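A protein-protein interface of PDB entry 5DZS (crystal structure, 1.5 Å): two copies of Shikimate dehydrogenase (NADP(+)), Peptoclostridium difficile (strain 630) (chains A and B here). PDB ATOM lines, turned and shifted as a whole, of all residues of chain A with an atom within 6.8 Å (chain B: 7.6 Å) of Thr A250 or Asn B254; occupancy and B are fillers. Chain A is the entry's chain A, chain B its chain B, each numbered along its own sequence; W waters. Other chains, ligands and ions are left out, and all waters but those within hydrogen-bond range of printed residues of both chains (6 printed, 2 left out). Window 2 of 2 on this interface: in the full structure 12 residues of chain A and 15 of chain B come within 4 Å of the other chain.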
ATOM      1  N   LEU A  27      17.152 -29.327  10.655  1.00  0.00           N
ATOM      2  CA  LEU A  27      16.670 -28.991  11.994  1.00  0.00           C
ATOM      3  C   LEU A  27      15.147 -28.882  12.110  1.00  0.00           C
ATOM      4  O   LEU A  27      14.648 -28.639  13.191  1.00  0.00           O
ATOM      5  CB  LEU A  27      17.316 -27.676  12.441  1.00  0.00           C
ATOM      6  CG  LEU A  27      18.837 -27.672  12.553  1.00  0.00           C
ATOM      7  CD1 LEU A  27      19.281 -26.253  12.938  1.00  0.00           C
ATOM      8  CD2 LEU A  27      19.328 -28.675  13.547  1.00  0.00           C
ATOM      9  N   ILE A  29      13.052 -26.571  11.038  1.00  0.00           N
ATOM     10  CA  ILE A  29      12.672 -25.209  11.437  1.00  0.00           C
ATOM     11  C   ILE A  29      11.891 -24.551  10.326  1.00  0.00           C
ATOM     12  O   ILE A  29      12.310 -24.579   9.171  1.00  0.00           O
ATOM     13  CB  ILE A  29      13.919 -24.361  11.703  1.00  0.00           C
ATOM     14  CG1 ILE A  29      14.708 -24.972  12.876  1.00  0.00           C
ATOM     15  CG2 ILE A  29      13.534 -22.893  11.953  1.00  0.00           C
ATOM     16  CD1 ILE A  29      16.034 -24.299  13.092  1.00  0.00           C
ATOM     17  N   ILE A 241      26.253 -21.736  10.128  1.00  0.00           N
ATOM     18  CA  ILE A 241      25.761 -22.424  11.323  1.00  0.00           C
ATOM     19  C   ILE A 241      25.938 -21.576  12.590  1.00  0.00           C
ATOM     20  O   ILE A 241      25.072 -21.574  13.486  1.00  0.00           O
ATOM     21  CB  ILE A 241      26.393 -23.809  11.439  1.00  0.00           C
ATOM     22  CG1 ILE A 241      25.981 -24.600  10.188  1.00  0.00           C
ATOM     23  CG2 ILE A 241      25.935 -24.484  12.727  1.00  0.00           C
ATOM     24  CD1 ILE A 241      26.813 -25.833   9.913  1.00  0.00           C
ATOM     25  N   GLN A 244      23.146 -19.151  12.557  1.00  0.00           N
ATOM     26  CA  GLN A 244      21.918 -19.807  12.996  1.00  0.00           C
ATOM     27  C   GLN A 244      21.883 -20.014  14.523  1.00  0.00           C
ATOM     28  O   GLN A 244      20.831 -19.876  15.148  1.00  0.00           O
ATOM     29  CB  GLN A 244      21.723 -21.125  12.235  1.00  0.00           C
ATOM     30  CG  GLN A 244      21.317 -20.891  10.802  1.00  0.00           C
ATOM     31  CD  GLN A 244      19.941 -20.283  10.649  1.00  0.00           C
ATOM     32  OE1 GLN A 244      19.098 -20.252  11.568  1.00  0.00           O
ATOM     33  NE2 GLN A 244      19.709 -19.720   9.474  1.00  0.00           N
ATOM     34  N   GLU A 245      23.015 -20.315  15.135  1.00  0.00           N
ATOM     35  CA  GLU A 245      23.030 -20.434  16.595  1.00  0.00           C
ATOM     36  C   GLU A 245      22.635 -19.127  17.233  1.00  0.00           C
ATOM     37  O   GLU A 245      21.924 -19.093  18.223  1.00  0.00           O
ATOM     38  CB  GLU A 245      24.401 -20.868  17.113  1.00  0.00           C
ATOM     39  CG  GLU A 245      24.754 -22.319  16.836  1.00  0.00           C
ATOM     40  CD  GLU A 245      25.986 -22.754  17.587  1.00  0.00           C
ATOM     41  OE1 GLU A 245      26.917 -21.925  17.704  1.00  0.00           O
ATOM     42  OE2 GLU A 245      26.051 -23.925  18.071  1.00  0.00           O
ATOM     43  N   ILE A 246      23.181 -18.032  16.722  1.00  0.00           N
ATOM     44  CA  ILE A 246      22.837 -16.705  17.224  1.00  0.00           C
ATOM     45  C   ILE A 246      21.360 -16.370  17.008  1.00  0.00           C
ATOM     46  O   ILE A 246      20.649 -15.949  17.931  1.00  0.00           O
ATOM     47  CB  ILE A 246      23.705 -15.630  16.549  1.00  0.00           C
ATOM     48  CG1 ILE A 246      25.184 -15.811  16.956  1.00  0.00           C
ATOM     49  CG2 ILE A 246      23.184 -14.225  16.894  1.00  0.00           C
ATOM     50  CD1 ILE A 246      26.154 -14.998  16.100  1.00  0.00           C
ATOM     51  N   TRP A 247      20.876 -16.643  15.809  1.00  0.00           N
ATOM     52  CA  TRP A 247      19.497 -16.273  15.487  1.00  0.00           C
ATOM     53  C   TRP A 247      18.474 -17.129  16.227  1.00  0.00           C
ATOM     54  O   TRP A 247      17.436 -16.613  16.675  1.00  0.00           O
ATOM     55  CB  TRP A 247      19.259 -16.385  13.987  1.00  0.00           C
ATOM     56  CG  TRP A 247      20.013 -15.381  13.166  1.00  0.00           C
ATOM     57  CD1 TRP A 247      20.367 -14.123  13.536  1.00  0.00           C
ATOM     58  CD2 TRP A 247      20.477 -15.549  11.817  1.00  0.00           C
ATOM     59  NE1 TRP A 247      21.066 -13.516  12.531  1.00  0.00           N
ATOM     60  CE2 TRP A 247      21.119 -14.358  11.449  1.00  0.00           C
ATOM     61  CE3 TRP A 247      20.392 -16.587  10.891  1.00  0.00           C
ATOM     62  CZ2 TRP A 247      21.686 -14.185  10.198  1.00  0.00           C
ATOM     63  CZ3 TRP A 247      20.949 -16.412   9.636  1.00  0.00           C
ATOM     64  CH2 TRP A 247      21.584 -15.206   9.303  1.00  0.00           C
ATOM     65  N   GLN A 248      18.772 -18.428  16.325  1.00  0.00           N
ATOM     66  CA  GLN A 248      17.882 -19.413  17.010  1.00  0.00           C
ATOM     67  C   GLN A 248      18.142 -19.470  18.541  1.00  0.00           C
ATOM     68  O   GLN A 248      17.360 -20.105  19.295  1.00  0.00           O
ATOM     69  CB  GLN A 248      18.060 -20.817  16.401  1.00  0.00           C
ATOM     70  CG  GLN A 248      17.941 -20.927  14.876  1.00  0.00           C
ATOM     71  CD  GLN A 248      16.593 -20.487  14.331  1.00  0.00           C
ATOM     72  OE1 GLN A 248      15.559 -20.703  14.967  1.00  0.00           O
ATOM     73  NE2 GLN A 248      16.598 -19.889  13.146  1.00  0.00           N
ATOM     74  N   ASP A 249      19.198 -18.795  19.003  1.00  0.00           N
ATOM     75  CA  ASP A 249      19.631 -18.788  20.420  1.00  0.00           C
ATOM     76  C   ASP A 249      19.620 -20.210  20.944  1.00  0.00           C
ATOM     77  O   ASP A 249      19.005 -20.507  21.989  1.00  0.00           O
ATOM     78  CB  ASP A 249      18.836 -17.876  21.364  1.00  0.00           C
ATOM     79  CG  ASP A 249      19.518 -17.742  22.750  1.00  0.00           C
ATOM     80  OD1 ASP A 249      20.697 -18.175  22.936  1.00  0.00           O
ATOM     81  OD2 ASP A 249      18.849 -17.262  23.686  1.00  0.00           O
ATOM     82  N   THR A 250      20.332 -21.070  20.223  1.00  0.00           N
ATOM     83  CA  THR A 250      20.422 -22.458  20.615  1.00  0.00           C
ATOM     84  C   THR A 250      21.668 -23.082  20.003  1.00  0.00           C
ATOM     85  O   THR A 250      22.119 -22.658  18.955  1.00  0.00           O
ATOM     86  CB  THR A 250      19.141 -23.221  20.240  1.00  0.00           C
ATOM     87  OG1 THR A 250      19.076 -24.434  21.033  1.00  0.00           O
ATOM     88  CG2 THR A 250      19.082 -23.519  18.774  1.00  0.00           C
ATOM     89  N   LYS A 251      22.230 -24.069  20.702  1.00  0.00           N
ATOM     90  CA  LYS A 251      23.389 -24.803  20.221  1.00  0.00           C
ATOM     91  C   LYS A 251      22.977 -25.684  19.024  1.00  0.00           C
ATOM     92  O   LYS A 251      21.911 -26.343  19.052  1.00  0.00           O
ATOM     93  CB  LYS A 251      23.993 -25.664  21.334  1.00  0.00           C
ATOM     94  CG  LYS A 251      25.361 -26.243  20.994  1.00  0.00           C
ATOM     95  CD  LYS A 251      25.985 -26.966  22.173  1.00  0.00           C
ATOM     96  CE  LYS A 251      27.340 -27.550  21.777  1.00  0.00           C
ATOM     97  NZ  LYS A 251      27.892 -28.428  22.835  1.00  0.00           N
ATOM     98  N   ILE A 252      23.802 -25.694  17.997  1.00  0.00           N
ATOM     99  CA  ILE A 252      23.571 -26.529  16.821  1.00  0.00           C
ATOM    100  C   ILE A 252      24.711 -27.538  16.776  1.00  0.00           C
ATOM    101  O   ILE A 252      25.889 -27.175  16.862  1.00  0.00           O
ATOM    102  CB  ILE A 252      23.450 -25.703  15.529  1.00  0.00           C
ATOM    103  CG1 ILE A 252      22.200 -24.848  15.625  1.00  0.00           C
ATOM    104  CG2 ILE A 252      23.397 -26.643  14.316  1.00  0.00           C
ATOM    105  CD1 ILE A 252      22.071 -23.825  14.541  1.00  0.00           C
ATOM    106  N   TYR B 234      15.672 -22.731  39.809  1.00  0.00           N
ATOM    107  CA  TYR B 234      15.772 -23.005  38.378  1.00  0.00           C
ATOM    108  C   TYR B 234      16.272 -21.773  37.625  1.00  0.00           C
ATOM    109  O   TYR B 234      17.088 -21.866  36.711  1.00  0.00           O
ATOM    110  CB  TYR B 234      14.417 -23.479  37.825  1.00  0.00           C
ATOM    111  CG  TYR B 234      14.487 -24.120  36.468  1.00  0.00           C
ATOM    112  CD1 TYR B 234      14.856 -25.452  36.340  1.00  0.00           C
ATOM    113  CD2 TYR B 234      14.184 -23.410  35.313  1.00  0.00           C
ATOM    114  CE1 TYR B 234      14.915 -26.058  35.108  1.00  0.00           C
ATOM    115  CE2 TYR B 234      14.241 -24.022  34.063  1.00  0.00           C
ATOM    116  CZ  TYR B 234      14.606 -25.340  33.974  1.00  0.00           C
ATOM    117  OH  TYR B 234      14.678 -26.008  32.760  1.00  0.00           O
ATOM    118  N   ILE B 241      24.040 -20.287  33.401  1.00  0.00           N
ATOM    119  CA  ILE B 241      24.368 -20.851  32.089  1.00  0.00           C
ATOM    120  C   ILE B 241      24.347 -19.764  31.007  1.00  0.00           C
ATOM    121  O   ILE B 241      25.273 -19.701  30.173  1.00  0.00           O
ATOM    122  CB  ILE B 241      23.437 -22.043  31.775  1.00  0.00           C
ATOM    123  CG1 ILE B 241      23.775 -23.203  32.721  1.00  0.00           C
ATOM    124  CG2 ILE B 241      23.558 -22.486  30.317  1.00  0.00           C
ATOM    125  CD1 ILE B 241      22.748 -24.323  32.722  1.00  0.00           C
ATOM    126  N   LYS B 242      23.351 -18.893  31.027  1.00  0.00           N
ATOM    127  CA  LYS B 242      23.313 -17.801  30.068  1.00  0.00           C
ATOM    128  C   LYS B 242      24.531 -16.889  30.235  1.00  0.00           C
ATOM    129  O   LYS B 242      25.118 -16.432  29.255  1.00  0.00           O
ATOM    130  CB  LYS B 242      22.003 -17.015  30.209  1.00  0.00           C
ATOM    131  CG  LYS B 242      21.832 -15.895  29.202  1.00  0.00           C
ATOM    132  CD  LYS B 242      21.766 -16.384  27.764  1.00  0.00           C
ATOM    133  CE  LYS B 242      20.579 -17.291  27.461  1.00  0.00           C
ATOM    134  NZ  LYS B 242      20.516 -17.814  26.051  1.00  0.00           N
ATOM    135  N   GLU B 245      27.387 -18.525  28.606  1.00  0.00           N
ATOM    136  CA  GLU B 245      27.291 -18.457  27.150  1.00  0.00           C
ATOM    137  C   GLU B 245      27.852 -17.105  26.674  1.00  0.00           C
ATOM    138  O   GLU B 245      28.580 -17.018  25.705  1.00  0.00           O
ATOM    139  CB  GLU B 245      25.845 -18.603  26.664  1.00  0.00           C
ATOM    140  CG  GLU B 245      25.293 -20.016  26.803  1.00  0.00           C
ATOM    141  CD  GLU B 245      23.909 -20.152  26.216  1.00  0.00           C
ATOM    142  OE1 GLU B 245      23.599 -21.243  25.681  1.00  0.00           O
ATOM    143  OE2 GLU B 245      23.128 -19.196  26.234  1.00  0.00           O
ATOM    144  N   LYS B 251      27.286 -21.232  22.613  1.00  0.00           N
ATOM    145  CA  LYS B 251      26.043 -21.756  23.143  1.00  0.00           C
ATOM    146  C   LYS B 251      26.288 -23.077  23.892  1.00  0.00           C
ATOM    147  O   LYS B 251      27.153 -23.877  23.523  1.00  0.00           O
ATOM    148  CB  LYS B 251      25.010 -21.978  22.011  1.00  0.00           C
ATOM    149  CG  LYS B 251      24.661 -20.730  21.211  1.00  0.00           C
ATOM    150  CD  LYS B 251      24.036 -19.621  22.028  1.00  0.00           C
ATOM    151  CE  LYS B 251      23.628 -18.413  21.181  1.00  0.00           C
ATOM    152  NZ  LYS B 251      23.074 -17.271  21.961  1.00  0.00           N
ATOM    153  N   ILE B 252      25.524 -23.263  24.953  1.00  0.00           N
ATOM    154  CA  ILE B 252      25.592 -24.429  25.815  1.00  0.00           C
ATOM    155  C   ILE B 252      24.366 -25.332  25.587  1.00  0.00           C
ATOM    156  O   ILE B 252      23.224 -24.862  25.448  1.00  0.00           O
ATOM    157  CB  ILE B 252      25.760 -23.998  27.294  1.00  0.00           C
ATOM    158  CG1 ILE B 252      27.137 -23.372  27.478  1.00  0.00           C
ATOM    159  CG2 ILE B 252      25.599 -25.186  28.252  1.00  0.00           C
ATOM    160  CD1 ILE B 252      27.330 -22.634  28.802  1.00  0.00           C
ATOM    161  N   ASP B 253      24.635 -26.629  25.525  1.00  0.00           N
ATOM    162  CA  ASP B 253      23.607 -27.638  25.285  1.00  0.00           C
ATOM    163  C   ASP B 253      22.415 -27.458  26.238  1.00  0.00           C
ATOM    164  O   ASP B 253      22.609 -27.283  27.431  1.00  0.00           O
ATOM    165  CB  ASP B 253      24.238 -29.023  25.434  1.00  0.00           C
ATOM    166  CG  ASP B 253      23.309 -30.150  25.009  1.00  0.00           C
ATOM    167  OD1 ASP B 253      22.193 -30.251  25.541  1.00  0.00           O
ATOM    168  OD2 ASP B 253      23.717 -30.959  24.154  1.00  0.00           O
ATOM    169  N   ASN B 254      21.200 -27.487  25.686  1.00  0.00           N
ATOM    170  CA  ASN B 254      19.950 -27.290  26.471  1.00  0.00           C
ATOM    171  C   ASN B 254      19.776 -28.233  27.637  1.00  0.00           C
ATOM    172  O   ASN B 254      19.194 -27.875  28.655  1.00  0.00           O
ATOM    173  CB  ASN B 254      18.716 -27.476  25.583  1.00  0.00           C
ATOM    174  CG  ASN B 254      18.456 -26.294  24.682  1.00  0.00           C
ATOM    175  OD1 ASN B 254      18.985 -25.207  24.895  1.00  0.00           O
ATOM    176  ND2 ASN B 254      17.601 -26.495  23.679  1.00  0.00           N
ATOM    177  N   SER B 255      20.261 -29.449  27.472  1.00  0.00           N
ATOM    178  CA  SER B 255      20.098 -30.476  28.490  1.00  0.00           C
ATOM    179  C   SER B 255      20.872 -30.194  29.765  1.00  0.00           C
ATOM    180  O   SER B 255      20.543 -30.715  30.819  1.00  0.00           O
ATOM    181  CB  SER B 255      20.547 -31.810  27.927  1.00  0.00           C
ATOM    182  OG  SER B 255      21.921 -31.781  27.607  1.00  0.00           O
ATOM    183  N   ILE B 256      21.883 -29.333  29.692  1.00  0.00           N
ATOM    184  CA  ILE B 256      22.725 -29.058  30.856  1.00  0.00           C
ATOM    185  C   ILE B 256      21.982 -28.414  32.040  1.00  0.00           C
ATOM    186  O   ILE B 256      22.225 -28.739  33.197  1.00  0.00           O
ATOM    187  CB  ILE B 256      23.982 -28.267  30.445  1.00  0.00           C
ATOM    188  CG1 ILE B 256      24.849 -29.148  29.532  1.00  0.00           C
ATOM    189  CG2 ILE B 256      24.766 -27.812  31.665  1.00  0.00           C
ATOM    190  CD1 ILE B 256      26.122 -28.524  29.032  1.00  0.00           C
ATOM    191  N   LEU B 257      21.071 -27.475  31.767  1.00  0.00           N
ATOM    192  CA  LEU B 257      20.306 -26.838  32.820  1.00  0.00           C
ATOM    193  C   LEU B 257      19.577 -27.846  33.717  1.00  0.00           C
ATOM    194  O   LEU B 257      19.658 -27.758  34.942  1.00  0.00           O
ATOM    195  CB  LEU B 257      19.319 -25.869  32.161  1.00  0.00           C
ATOM    196  CG  LEU B 257      18.178 -25.263  32.971  1.00  0.00           C
ATOM    197  CD1 LEU B 257      18.638 -24.657  34.270  1.00  0.00           C
ATOM    198  CD2 LEU B 257      17.474 -24.221  32.111  1.00  0.00           C
ATOM    199  N   ASP B 258      18.847 -28.771  33.113  1.00  0.00           N
ATOM    200  CA  ASP B 258      18.122 -29.762  33.888  1.00  0.00           C
ATOM    201  C   ASP B 258      19.069 -30.676  34.641  1.00  0.00           C
ATOM    202  O   ASP B 258      18.791 -31.048  35.788  1.00  0.00           O
ATOM    203  CB  ASP B 258      17.168 -30.583  33.018  1.00  0.00           C
ATOM    204  CG  ASP B 258      15.918 -29.811  32.632  1.00  0.00           C
ATOM    205  OD1 ASP B 258      15.608 -28.789  33.293  1.00  0.00           O
ATOM    206  OD2 ASP B 258      15.236 -30.239  31.674  1.00  0.00           O
ATOM    207  N   VAL B 259      20.168 -31.071  34.005  1.00  0.00           N
ATOM    208  CA  VAL B 259      21.124 -31.952  34.676  1.00  0.00           C
ATOM    209  C   VAL B 259      21.669 -31.238  35.914  1.00  0.00           C
ATOM    210  O   VAL B 259      21.677 -31.780  37.021  1.00  0.00           O
ATOM    211  CB  VAL B 259      22.273 -32.379  33.728  1.00  0.00           C
ATOM    212  CG1 VAL B 259      23.341 -33.143  34.483  1.00  0.00           C
ATOM    213  CG2 VAL B 259      21.725 -33.237  32.593  1.00  0.00           C
HETATM  214  O   HOH W   1      17.939 -22.926  23.231  1.00  0.00           O
HETATM  215  O   HOH W   2      27.326 -27.548  25.682  1.00  0.00           O
HETATM  216  O   HOH W   3      26.030 -31.097  22.674  1.00  0.00           O
HETATM  217  O   HOH W   4      27.596 -20.004  19.501  1.00  0.00           O
HETATM  218  O   HOH W   5      21.427 -15.325  20.456  1.00  0.00           O
HETATM  219  O   HOH W   6      28.500 -22.498  20.229  1.00  0.00           O
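O of Glu A245 lies within hydrogen-bond range of N of Thr A250, at 3.2 Å. The backbone NH (N) of Ile A252 lies within hydrogen-bond range of the side-chain carboxylate (OE2) of Glu A245 (2.9 Å). The side-chain amino group (NZ) of Lys B242 is in salt-bridge range of the side-chain carboxylate (OE2) of Glu B245 (3.0 Å). The side-chain hydroxyl of Ser B255 sits at hydrogen-bond distance from the side-chain carboxylate of Asp B253 (2.6 Å).
Printed residues of chain B within 4 Å of Glu A245: Lys B251. Of the printed residues of chain B, Asp A249 touches Lys B242 and Lys B251. Thr A250 touches just these residues of chain B: Lys B251 (3.9 Å) and Asn B254 (3.7 Å). Printed residues of chain A within 4 Å of Lys B242: Asp A249 (2.9 Å). Printed residues of chain A within 4 Å of Lys B251: Glu A245, Asp A249, Thr A250 and Lys A251. Of the printed residues of chain A, Asp B253 touches Lys A251 (3.6 Å). Asn B254 touches just one residue of chain A: Thr A250 (3.7 Å). The nearest residue of chain B that does not touch Thr A250 is Ile B252 (5.9 Å). The nearest printed residue of chain B that does not touch Asp A249 is Glu B245 (4.2 Å).
Glu A245 touches Lys B251, but with the chains exchanged Lys A251 does not touch Glu B245 (5.9 Å). Lys B251 touches its own counterpart, Lys A251. 4 positions are printed for both chains. Of the 7 pairs that touch across the chains among the printed residues, 1 has its exchanged pair printed and touching as well.
Among the printed residues, merely in contact across the chains: Glu A245 with Lys B251 (3.5 Å), Thr A250 with Lys B251 (3.9 Å), Thr A250 with Asn B254 (3.7 Å), Lys A251 with Lys B251 (3.6 Å) and Lys A251 with Asp B253 (3.6 Å).
Of the 12 printed residues of chain A, 4 touch a printed residue of chain B. Among the printed residues, Asp or Glu carboxylates within 4 Å of a Lys or Arg side-chain nitrogen of the other chain: Asp A249 with Lys B242 and Asp A249 with Lys B251.
Water W5 bridges O of Ile A246 (2.7 Å) and NZ of Lys B251 (3.0 Å). Water W4 lies within hydrogen-bond range of OE1 of Glu A245 (2.7 Å) and N of Lys B251 (3.4 Å). Water W3 lies within hydrogen-bond range of OD2 of Asp B253 (2.7 Å) and NZ of Lys A251 (3.3 Å). Water W2 bridges N of Asp B253 and NZ of Lys A251. Water W1 lies within hydrogen-bond range of OG1 of Thr A250 (2.9 Å), O of Asp A249 (2.9 Å) and OD1 of Asn B254 (3.0 Å). Water W6 bridges the backbone NH (N) of Lys B251 (3.0 Å) and the side-chain carboxylate (OE1) of Glu A245 (3.0 Å).
OD2 of Asp A249 lies within salt-bridge range of NZ of Lys B242 (2.9 Å). OD1 of Asp A249 is in salt-bridge range of NZ of Lys B251 (2.7 Å).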
